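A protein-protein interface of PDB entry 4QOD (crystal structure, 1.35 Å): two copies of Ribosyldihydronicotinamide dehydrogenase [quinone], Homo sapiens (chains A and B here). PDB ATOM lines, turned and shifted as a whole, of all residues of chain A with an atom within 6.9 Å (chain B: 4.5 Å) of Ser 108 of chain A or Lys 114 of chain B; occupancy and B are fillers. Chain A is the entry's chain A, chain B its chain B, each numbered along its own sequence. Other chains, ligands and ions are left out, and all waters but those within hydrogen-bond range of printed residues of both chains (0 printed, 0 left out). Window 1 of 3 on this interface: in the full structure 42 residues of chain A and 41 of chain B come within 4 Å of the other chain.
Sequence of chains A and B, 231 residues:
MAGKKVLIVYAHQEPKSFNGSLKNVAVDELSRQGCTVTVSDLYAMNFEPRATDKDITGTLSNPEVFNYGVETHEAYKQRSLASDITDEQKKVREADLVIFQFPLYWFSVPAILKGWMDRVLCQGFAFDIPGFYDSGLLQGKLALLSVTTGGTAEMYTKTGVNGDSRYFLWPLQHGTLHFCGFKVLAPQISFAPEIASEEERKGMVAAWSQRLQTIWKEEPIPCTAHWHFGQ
O of Tyr 105 of chain A sits at hydrogen-bond distance from NZ of Lys 114 of chain B, at 2.9 Å. The backbone carbonyl oxygen (O) of Met 117 of chain B lies within hydrogen-bond range of the indole nitrogen (NE1) of Trp 106 of chain A (3.1 Å). The backbone carbonyl oxygen (O) of Val 109 of chain A sits at hydrogen-bond distance from the side-chain amino group (NZ) of Lys 114 of chain B, at 2.7 Å. The backbone NH (N) of Ala 111 of chain A sits at hydrogen-bond distance from the side-chain carboxylate (OD2) of Asp 118 of chain B. The backbone carbonyl oxygen of Val 109 of chain B is in hydrogen-bond range of the side-chain amino group of Lys 114 of chain A (2.8 Å).
NZ of Lys 114 of chain B is in salt-bridge range of OD1 of Asp 118 of chain B, 2.7 Å away.
Asp 118 of chain B touches Tyr 105 of chain A (OD2 to CD2, 3.6 Å). OD1 of Asp 118 of chain B touches CD1 of Trp 106 of chain A, 3.5 Å away. CB of Ser 108 of chain A touches CE of Lys 114 of chain B (3.7 Å). Pro 110 of chain A touches Asp 118 of chain B (C to OD2, 3.8 Å). O of Ala 111 of chain B touches CB of Ala 111 of chain A, 3.6 Å away. Ala 111 of chain A touches Lys 114 of chain B (CB to C, 3.9 Å). Gly 115 of chain B touches Ala 111 of chain A. Lys 114 of chain A touches Ala 111 of chain B (C to CB, 3.9 Å). N of Gly 115 of chain A touches CB of Ala 111 of chain B (3.4 Å).
Lys 114 of chain B touches just these residues of chain A: Tyr 105, Ser 108, Val 109 and Ala 111. Printed residues of chain B within 4 Å of Trp 106 of chain A: Met 117 (3.1 Å) and Asp 118 (3.5 Å). Of the printed residues of chain B, Tyr 105 of chain A touches Lys 114 and Asp 118. Of the printed residues of chain B, Ala 111 of chain A touches Ala 111, Lys 114, Gly 115 and Asp 118.
Hydrophobic or aromatic side chains of chain A within 4 Å of the printed part of chain B: Tyr 105, Trp 106 and Ala 111. Along chain A the printed residues that touch a printed residue of chain B span positions 105 to 115. Of the 10 printed residues of chain B, 6 touch a printed residue of chain A. Among the printed residues, no Asp or Glu carboxylate lies within 4 Å of a Lys or Arg side-chain nitrogen of the other chain.
Val 109 of chain A touches Lys 114 of chain B, and with the chains exchanged Lys 114 of chain A touches Val 109 of chain B. Ala 111 of chain A touches its own counterpart, Ala 111 of chain B. Ala 111 of chain A touches Lys 114 of chain B, and with the chains exchanged Lys 114 of chain A touches Ala 111 of chain B. Ala 111 of chain A touches Gly 115 of chain B, and with the chains exchanged Gly 115 of chain A touches Ala 111 of chain B. Positions printed for both chains: 109, 110, 111, 112, 114 and 115. Of the 14 pairs that touch across the chains among the printed residues, 7 have their exchanged pair printed and touching as well.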
ATOM      1  N   PHE A 102       5.534  -0.405  -0.382  1.00  0.00           N
ATOM      2  CA  PHE A 102       6.849  -0.023   0.127  1.00  0.00           C
ATOM      3  C   PHE A 102       6.914   1.484   0.405  1.00  0.00           C
ATOM      4  O   PHE A 102       6.312   2.280  -0.315  1.00  0.00           O
ATOM      5  CB  PHE A 102       7.980  -0.401  -0.870  1.00  0.00           C
ATOM      6  CG  PHE A 102       7.862   0.217  -2.237  1.00  0.00           C
ATOM      7  CD1 PHE A 102       7.032  -0.333  -3.214  1.00  0.00           C
ATOM      8  CD2 PHE A 102       8.571   1.332  -2.554  1.00  0.00           C
ATOM      9  CE1 PHE A 102       6.933   0.261  -4.440  1.00  0.00           C
ATOM     10  CE2 PHE A 102       8.425   1.948  -3.763  1.00  0.00           C
ATOM     11  CZ  PHE A 102       7.623   1.416  -4.731  1.00  0.00           C
ATOM     12  N   PRO A 103       7.836   1.860   1.313  1.00  0.00           N
ATOM     13  CA  PRO A 103       8.237   3.251   1.443  1.00  0.00           C
ATOM     14  C   PRO A 103       9.278   3.594   0.399  1.00  0.00           C
ATOM     15  O   PRO A 103      10.153   2.786   0.066  1.00  0.00           O
ATOM     16  CB  PRO A 103       8.880   3.293   2.823  1.00  0.00           C
ATOM     17  CG  PRO A 103       9.470   1.894   2.999  1.00  0.00           C
ATOM     18  CD  PRO A 103       8.502   0.964   2.287  1.00  0.00           C
ATOM     19  N   LEU A 104       9.221   4.816  -0.098  1.00  0.00           N
ATOM     20  CA  LEU A 104      10.187   5.302  -1.093  1.00  0.00           C
ATOM     21  C   LEU A 104      11.544   5.558  -0.417  1.00  0.00           C
ATOM     22  O   LEU A 104      11.619   6.387   0.512  1.00  0.00           O
ATOM     23  CB  LEU A 104       9.691   6.611  -1.692  1.00  0.00           C
ATOM     24  CG  LEU A 104      10.377   7.129  -2.958  1.00  0.00           C
ATOM     25  CD1 LEU A 104      10.003   6.259  -4.118  1.00  0.00           C
ATOM     26  CD2 LEU A 104      10.014   8.620  -3.210  1.00  0.00           C
ATOM     27  N   TYR A 105      12.573   4.818  -0.847  1.00  0.00           N
ATOM     28  CA  TYR A 105      13.950   4.976  -0.395  1.00  0.00           C
ATOM     29  C   TYR A 105      14.721   5.490  -1.531  1.00  0.00           C
ATOM     30  O   TYR A 105      14.890   4.830  -2.541  1.00  0.00           O
ATOM     31  CB  TYR A 105      14.547   3.634   0.117  1.00  0.00           C
ATOM     32  CG  TYR A 105      14.184   3.117   1.493  1.00  0.00           C
ATOM     33  CD1 TYR A 105      13.094   3.592   2.208  1.00  0.00           C
ATOM     34  CD2 TYR A 105      14.899   2.128   2.122  1.00  0.00           C
ATOM     35  CE1 TYR A 105      12.799   3.113   3.476  1.00  0.00           C
ATOM     36  CE2 TYR A 105      14.599   1.637   3.351  1.00  0.00           C
ATOM     37  CZ  TYR A 105      13.518   2.136   4.021  1.00  0.00           C
ATOM     38  OH  TYR A 105      13.203   1.589   5.233  1.00  0.00           O
ATOM     39  N   TRP A 106      15.224   6.744  -1.404  1.00  0.00           N
ATOM     40  CA  TRP A 106      16.029   7.322  -2.473  1.00  0.00           C
ATOM     41  C   TRP A 106      15.388   7.304  -3.849  1.00  0.00           C
ATOM     42  O   TRP A 106      15.944   6.886  -4.858  1.00  0.00           O
ATOM     43  CB  TRP A 106      17.477   6.704  -2.533  1.00  0.00           C
ATOM     44  CG  TRP A 106      18.247   7.011  -1.267  1.00  0.00           C
ATOM     45  CD1 TRP A 106      18.912   6.140  -0.460  1.00  0.00           C
ATOM     46  CD2 TRP A 106      18.543   8.312  -0.771  1.00  0.00           C
ATOM     47  NE1 TRP A 106      19.518   6.790   0.541  1.00  0.00           N
ATOM     48  CE2 TRP A 106      19.303   8.132   0.405  1.00  0.00           C
ATOM     49  CE3 TRP A 106      18.177   9.588  -1.156  1.00  0.00           C
ATOM     50  CZ2 TRP A 106      19.717   9.223   1.219  1.00  0.00           C
ATOM     51  CZ3 TRP A 106      18.580  10.654  -0.393  1.00  0.00           C
ATOM     52  CH2 TRP A 106      19.334  10.485   0.777  1.00  0.00           C
ATOM     53  N   PHE A 107      14.155   7.784  -3.871  1.00  0.00           N
ATOM     54  CA  PHE A 107      13.354   7.893  -5.091  1.00  0.00           C
ATOM     55  C   PHE A 107      13.135   6.496  -5.747  1.00  0.00           C
ATOM     56  O   PHE A 107      12.959   6.425  -6.890  1.00  0.00           O
ATOM     57  CB  PHE A 107      14.013   8.800  -6.144  1.00  0.00           C
ATOM     58  CG  PHE A 107      13.748  10.307  -6.031  1.00  0.00           C
ATOM     59  CD1 PHE A 107      13.463  10.920  -4.852  1.00  0.00           C
ATOM     60  CD2 PHE A 107      13.913  11.085  -7.155  1.00  0.00           C
ATOM     61  CE1 PHE A 107      13.285  12.308  -4.800  1.00  0.00           C
ATOM     62  CE2 PHE A 107      13.752  12.465  -7.107  1.00  0.00           C
ATOM     63  CZ  PHE A 107      13.444  13.066  -5.925  1.00  0.00           C
ATOM     64  N   SER A 108      13.212   5.439  -4.966  1.00  0.00           N
ATOM     65  CA  SER A 108      13.136   4.070  -5.478  1.00  0.00           C
ATOM     66  C   SER A 108      12.602   3.101  -4.421  1.00  0.00           C
ATOM     67  O   SER A 108      12.113   3.498  -3.433  1.00  0.00           O
ATOM     68  CB  SER A 108      14.529   3.655  -5.980  1.00  0.00           C
ATOM     69  OG  SER A 108      14.549   2.397  -6.616  1.00  0.00           O
ATOM     70  N   VAL A 109      12.754   1.806  -4.670  1.00  0.00           N
ATOM     71  CA  VAL A 109      12.357   0.781  -3.729  1.00  0.00           C
ATOM     72  C   VAL A 109      13.511   0.528  -2.714  1.00  0.00           C
ATOM     73  O   VAL A 109      14.683   0.760  -3.007  1.00  0.00           O
ATOM     74  CB  VAL A 109      12.082  -0.564  -4.443  1.00  0.00           C
ATOM     75  CG1 VAL A 109      10.801  -0.442  -5.273  1.00  0.00           C
ATOM     76  CG2 VAL A 109      13.213  -1.009  -5.386  1.00  0.00           C
ATOM     77  N   PRO A 110      13.144   0.165  -1.474  1.00  0.00           N
ATOM     78  CA  PRO A 110      14.165  -0.348  -0.560  1.00  0.00           C
ATOM     79  C   PRO A 110      15.024  -1.453  -1.192  1.00  0.00           C
ATOM     80  O   PRO A 110      14.507  -2.269  -1.970  1.00  0.00           O
ATOM     81  CB  PRO A 110      13.360  -0.866   0.627  1.00  0.00           C
ATOM     82  CG  PRO A 110      12.050  -0.109   0.553  1.00  0.00           C
ATOM     83  CD  PRO A 110      11.794  -0.006  -0.932  1.00  0.00           C
ATOM     84  N   ALA A 111      16.306  -1.517  -0.816  1.00  0.00           N
ATOM     85  CA  ALA A 111      17.186  -2.514  -1.426  1.00  0.00           C
ATOM     86  C   ALA A 111      16.651  -3.916  -1.304  1.00  0.00           C
ATOM     87  O   ALA A 111      16.933  -4.699  -2.207  1.00  0.00           O
ATOM     88  CB  ALA A 111      18.589  -2.449  -0.818  1.00  0.00           C
ATOM     89  N   ILE A 112      15.979  -4.313  -0.237  1.00  0.00           N
ATOM     90  CA  ILE A 112      15.455  -5.671  -0.149  1.00  0.00           C
ATOM     91  C   ILE A 112      14.531  -6.004  -1.332  1.00  0.00           C
ATOM     92  O   ILE A 112      14.542  -7.086  -1.885  1.00  0.00           O
ATOM     93  CB  ILE A 112      14.904  -6.031   1.213  1.00  0.00           C
ATOM     94  CG1 ILE A 112      14.781  -7.569   1.422  1.00  0.00           C
ATOM     95  CG2 ILE A 112      13.584  -5.250   1.481  1.00  0.00           C
ATOM     96  CD1 ILE A 112      14.437  -7.937   2.842  1.00  0.00           C
ATOM     97  N   LYS A 114      14.519  -4.162  -4.218  1.00  0.00           N
ATOM     98  CA  LYS A 114      15.288  -4.111  -5.440  1.00  0.00           C
ATOM     99  C   LYS A 114      15.872  -5.480  -5.671  1.00  0.00           C
ATOM    100  O   LYS A 114      16.000  -5.921  -6.804  1.00  0.00           O
ATOM    101  CB  LYS A 114      16.429  -3.076  -5.363  1.00  0.00           C
ATOM    102  CG  LYS A 114      17.194  -2.864  -6.624  1.00  0.00           C
ATOM    103  CD  LYS A 114      16.329  -2.622  -7.844  1.00  0.00           C
ATOM    104  CE  LYS A 114      17.050  -2.001  -8.982  1.00  0.00           C
ATOM    105  NZ  LYS A 114      18.184  -2.851  -9.492  1.00  0.00           N
ATOM    106  N   GLY A 115      16.354  -6.177  -4.646  1.00  0.00           N
ATOM    107  CA  GLY A 115      16.881  -7.473  -4.794  1.00  0.00           C
ATOM    108  C   GLY A 115      15.891  -8.494  -5.245  1.00  0.00           C
ATOM    109  O   GLY A 115      16.228  -9.401  -6.022  1.00  0.00           O
ATOM    110  N   VAL A 147       3.039   3.166  -2.843  1.00  0.00           N
ATOM    111  CA  VAL A 147       4.224   3.778  -2.282  1.00  0.00           C
ATOM    112  C   VAL A 147       3.877   4.793  -1.191  1.00  0.00           C
ATOM    113  O   VAL A 147       2.842   5.510  -1.306  1.00  0.00           O
ATOM    114  CB  VAL A 147       5.098   4.362  -3.440  1.00  0.00           C
ATOM    115  CG1 VAL A 147       4.301   5.183  -4.395  1.00  0.00           C
ATOM    116  CG2 VAL A 147       6.343   5.124  -2.936  1.00  0.00           C
ATOM    117  N   PHE A 168      10.126   9.708 -10.891  1.00  0.00           N
ATOM    118  CA  PHE A 168      10.840   8.610 -10.223  1.00  0.00           C
ATOM    119  C   PHE A 168      10.199   7.276 -10.481  1.00  0.00           C
ATOM    120  O   PHE A 168      10.793   6.225 -10.254  1.00  0.00           O
ATOM    121  CB  PHE A 168      11.063   8.962  -8.734  1.00  0.00           C
ATOM    122  CG  PHE A 168       9.842   8.901  -7.847  1.00  0.00           C
ATOM    123  CD1 PHE A 168       9.071   7.772  -7.676  1.00  0.00           C
ATOM    124  CD2 PHE A 168       9.427  10.091  -7.168  1.00  0.00           C
ATOM    125  CE1 PHE A 168       7.947   7.776  -6.812  1.00  0.00           C
ATOM    126  CE2 PHE A 168       8.335  10.099  -6.329  1.00  0.00           C
ATOM    127  CZ  PHE A 168       7.583   8.957  -6.166  1.00  0.00           C
ATOM    128  N   PRO A 171      11.913   4.154 -13.749  1.00  0.00           N
ATOM    129  CA  PRO A 171      12.664   2.916 -13.701  1.00  0.00           C
ATOM    130  C   PRO A 171      11.877   1.691 -13.275  1.00  0.00           C
ATOM    131  O   PRO A 171      12.167   0.579 -13.687  1.00  0.00           O
ATOM    132  CB  PRO A 171      13.826   3.218 -12.738  1.00  0.00           C
ATOM    133  CG  PRO A 171      13.931   4.688 -12.748  1.00  0.00           C
ATOM    134  CD  PRO A 171      12.513   5.203 -12.933  1.00  0.00           C
ATOM    135  N   LEU A 172      10.914   1.922 -12.422  1.00  0.00           N
ATOM    136  CA  LEU A 172      10.072   0.882 -11.844  1.00  0.00           C
ATOM    137  C   LEU A 172       8.943   0.436 -12.751  1.00  0.00           C
ATOM    138  O   LEU A 172       8.834  -0.723 -13.167  1.00  0.00           O
ATOM    139  CB  LEU A 172       9.533   1.332 -10.500  1.00  0.00           C
ATOM    140  CG  LEU A 172      10.573   1.690  -9.395  1.00  0.00           C
ATOM    141  CD1 LEU A 172       9.981   2.310  -8.136  1.00  0.00           C
ATOM    142  CD2 LEU A 172      11.345   0.461  -9.003  1.00  0.00           C
ATOM    143  N   VAL B 109      20.755   0.892  -9.814  1.00  0.00           N
ATOM    144  CA  VAL B 109      21.915   0.223  -9.228  1.00  0.00           C
ATOM    145  C   VAL B 109      21.549  -1.237  -8.821  1.00  0.00           C
ATOM    146  O   VAL B 109      20.402  -1.480  -8.451  1.00  0.00           O
ATOM    147  CB  VAL B 109      22.447   0.959  -8.013  1.00  0.00           C
ATOM    148  CG1 VAL B 109      23.146   2.268  -8.476  1.00  0.00           C
ATOM    149  CG2 VAL B 109      21.419   1.246  -6.926  1.00  0.00           C
ATOM    150  N   PRO B 110      22.497  -2.192  -8.917  1.00  0.00           N
ATOM    151  CA  PRO B 110      22.275  -3.491  -8.266  1.00  0.00           C
ATOM    152  C   PRO B 110      21.839  -3.301  -6.809  1.00  0.00           C
ATOM    153  O   PRO B 110      22.290  -2.395  -6.087  1.00  0.00           O
ATOM    154  CB  PRO B 110      23.637  -4.137  -8.323  1.00  0.00           C
ATOM    155  CG  PRO B 110      24.331  -3.460  -9.453  1.00  0.00           C
ATOM    156  CD  PRO B 110      23.873  -2.026  -9.414  1.00  0.00           C
ATOM    157  N   ALA B 111      21.005  -4.219  -6.261  1.00  0.00           N
ATOM    158  CA  ALA B 111      20.522  -4.100  -4.916  1.00  0.00           C
ATOM    159  C   ALA B 111      21.640  -3.958  -3.894  1.00  0.00           C
ATOM    160  O   ALA B 111      21.397  -3.297  -2.905  1.00  0.00           O
ATOM    161  CB  ALA B 111      19.647  -5.324  -4.623  1.00  0.00           C
ATOM    162  N   ILE B 112      22.804  -4.635  -4.048  1.00  0.00           N
ATOM    163  CA  ILE B 112      23.816  -4.478  -3.010  1.00  0.00           C
ATOM    164  C   ILE B 112      24.249  -3.026  -2.897  1.00  0.00           C
ATOM    165  O   ILE B 112      24.489  -2.519  -1.753  1.00  0.00           O
ATOM    166  CB  ILE B 112      25.023  -5.461  -3.262  1.00  0.00           C
ATOM    167  CG1 ILE B 112      25.843  -5.633  -1.991  1.00  0.00           C
ATOM    168  CG2 ILE B 112      25.814  -5.079  -4.523  1.00  0.00           C
ATOM    169  CD1 ILE B 112      26.879  -6.751  -2.127  1.00  0.00           C
ATOM    170  N   LEU B 113      24.338  -2.325  -4.046  1.00  0.00           N
ATOM    171  CA  LEU B 113      24.666  -0.883  -4.014  1.00  0.00           C
ATOM    172  C   LEU B 113      23.512  -0.036  -3.603  1.00  0.00           C
ATOM    173  O   LEU B 113      23.691   0.936  -2.858  1.00  0.00           O
ATOM    174  CB  LEU B 113      25.222  -0.504  -5.395  1.00  0.00           C
ATOM    175  CG  LEU B 113      25.554   0.963  -5.654  1.00  0.00           C
ATOM    176  CD1 LEU B 113      26.433   1.503  -4.532  1.00  0.00           C
ATOM    177  CD2 LEU B 113      26.139   1.107  -7.028  1.00  0.00           C
ATOM    178  N   LYS B 114      22.276  -0.429  -3.957  1.00  0.00           N
ATOM    179  CA  LYS B 114      21.132   0.288  -3.388  1.00  0.00           C
ATOM    180  C   LYS B 114      21.184   0.249  -1.866  1.00  0.00           C
ATOM    181  O   LYS B 114      20.846   1.219  -1.186  1.00  0.00           O
ATOM    182  CB  LYS B 114      19.817  -0.283  -3.902  1.00  0.00           C
ATOM    183  CG  LYS B 114      18.607   0.503  -3.490  1.00  0.00           C
ATOM    184  CD  LYS B 114      18.701   2.001  -3.818  1.00  0.00           C
ATOM    185  CE  LYS B 114      17.376   2.702  -3.807  1.00  0.00           C
ATOM    186  NZ  LYS B 114      16.657   2.586  -2.503  1.00  0.00           N
ATOM    187  N   GLY B 115      21.573  -0.909  -1.306  1.00  0.00           N
ATOM    188  CA  GLY B 115      21.666  -1.042   0.100  1.00  0.00           C
ATOM    189  C   GLY B 115      22.748  -0.191   0.730  1.00  0.00           C
ATOM    190  O   GLY B 115      22.523   0.335   1.860  1.00  0.00           O
ATOM    191  N   TRP B 116      23.871  -0.028   0.087  1.00  0.00           N
ATOM    192  CA  TRP B 116      24.855   0.935   0.499  1.00  0.00           C
ATOM    193  C   TRP B 116      24.255   2.331   0.487  1.00  0.00           C
ATOM    194  O   TRP B 116      24.356   3.038   1.497  1.00  0.00           O
ATOM    195  CB  TRP B 116      26.096   0.832  -0.400  1.00  0.00           C
ATOM    196  CG  TRP B 116      27.293   1.681  -0.005  1.00  0.00           C
ATOM    197  CD1 TRP B 116      28.440   1.279   0.625  1.00  0.00           C
ATOM    198  CD2 TRP B 116      27.488   3.097  -0.245  1.00  0.00           C
ATOM    199  NE1 TRP B 116      29.285   2.314   0.789  1.00  0.00           N
ATOM    200  CE2 TRP B 116      28.779   3.428   0.317  1.00  0.00           C
ATOM    201  CE3 TRP B 116      26.748   4.077  -0.821  1.00  0.00           C
ATOM    202  CZ2 TRP B 116      29.290   4.690   0.261  1.00  0.00           C
ATOM    203  CZ3 TRP B 116      27.264   5.350  -0.863  1.00  0.00           C
ATOM    204  CH2 TRP B 116      28.510   5.648  -0.311  1.00  0.00           C
ATOM    205  N   MET B 117      23.551   2.735  -0.441  1.00  0.00           N
ATOM    206  CA  MET B 117      22.952   4.053  -0.384  1.00  0.00           C
ATOM    207  C   MET B 117      21.944   4.178   0.742  1.00  0.00           C
ATOM    208  O   MET B 117      21.961   5.197   1.436  1.00  0.00           O
ATOM    209  CB  MET B 117      22.325   4.295  -1.751  1.00  0.00           C
ATOM    210  CG  MET B 117      23.288   4.585  -2.840  1.00  0.00           C
ATOM    211  SD  MET B 117      22.668   4.419  -4.502  1.00  0.00           S
ATOM    212  CE  MET B 117      24.045   5.137  -5.427  1.00  0.00           C
ATOM    213  N   ASP B 118      21.091   3.235   0.900  1.00  0.00           N
ATOM    214  CA  ASP B 118      20.032   3.218   1.876  1.00  0.00           C
ATOM    215  C   ASP B 118      20.613   3.273   3.275  1.00  0.00           C
ATOM    216  O   ASP B 118      20.113   3.966   4.097  1.00  0.00           O
ATOM    217  CB  ASP B 118      19.146   1.948   1.812  1.00  0.00           C
ATOM    218  CG  ASP B 118      18.258   1.850   0.544  1.00  0.00           C
ATOM    219  OD1 ASP B 118      18.140   2.786  -0.197  1.00  0.00           O
ATOM    220  OD2 ASP B 118      17.720   0.774   0.384  1.00  0.00           O
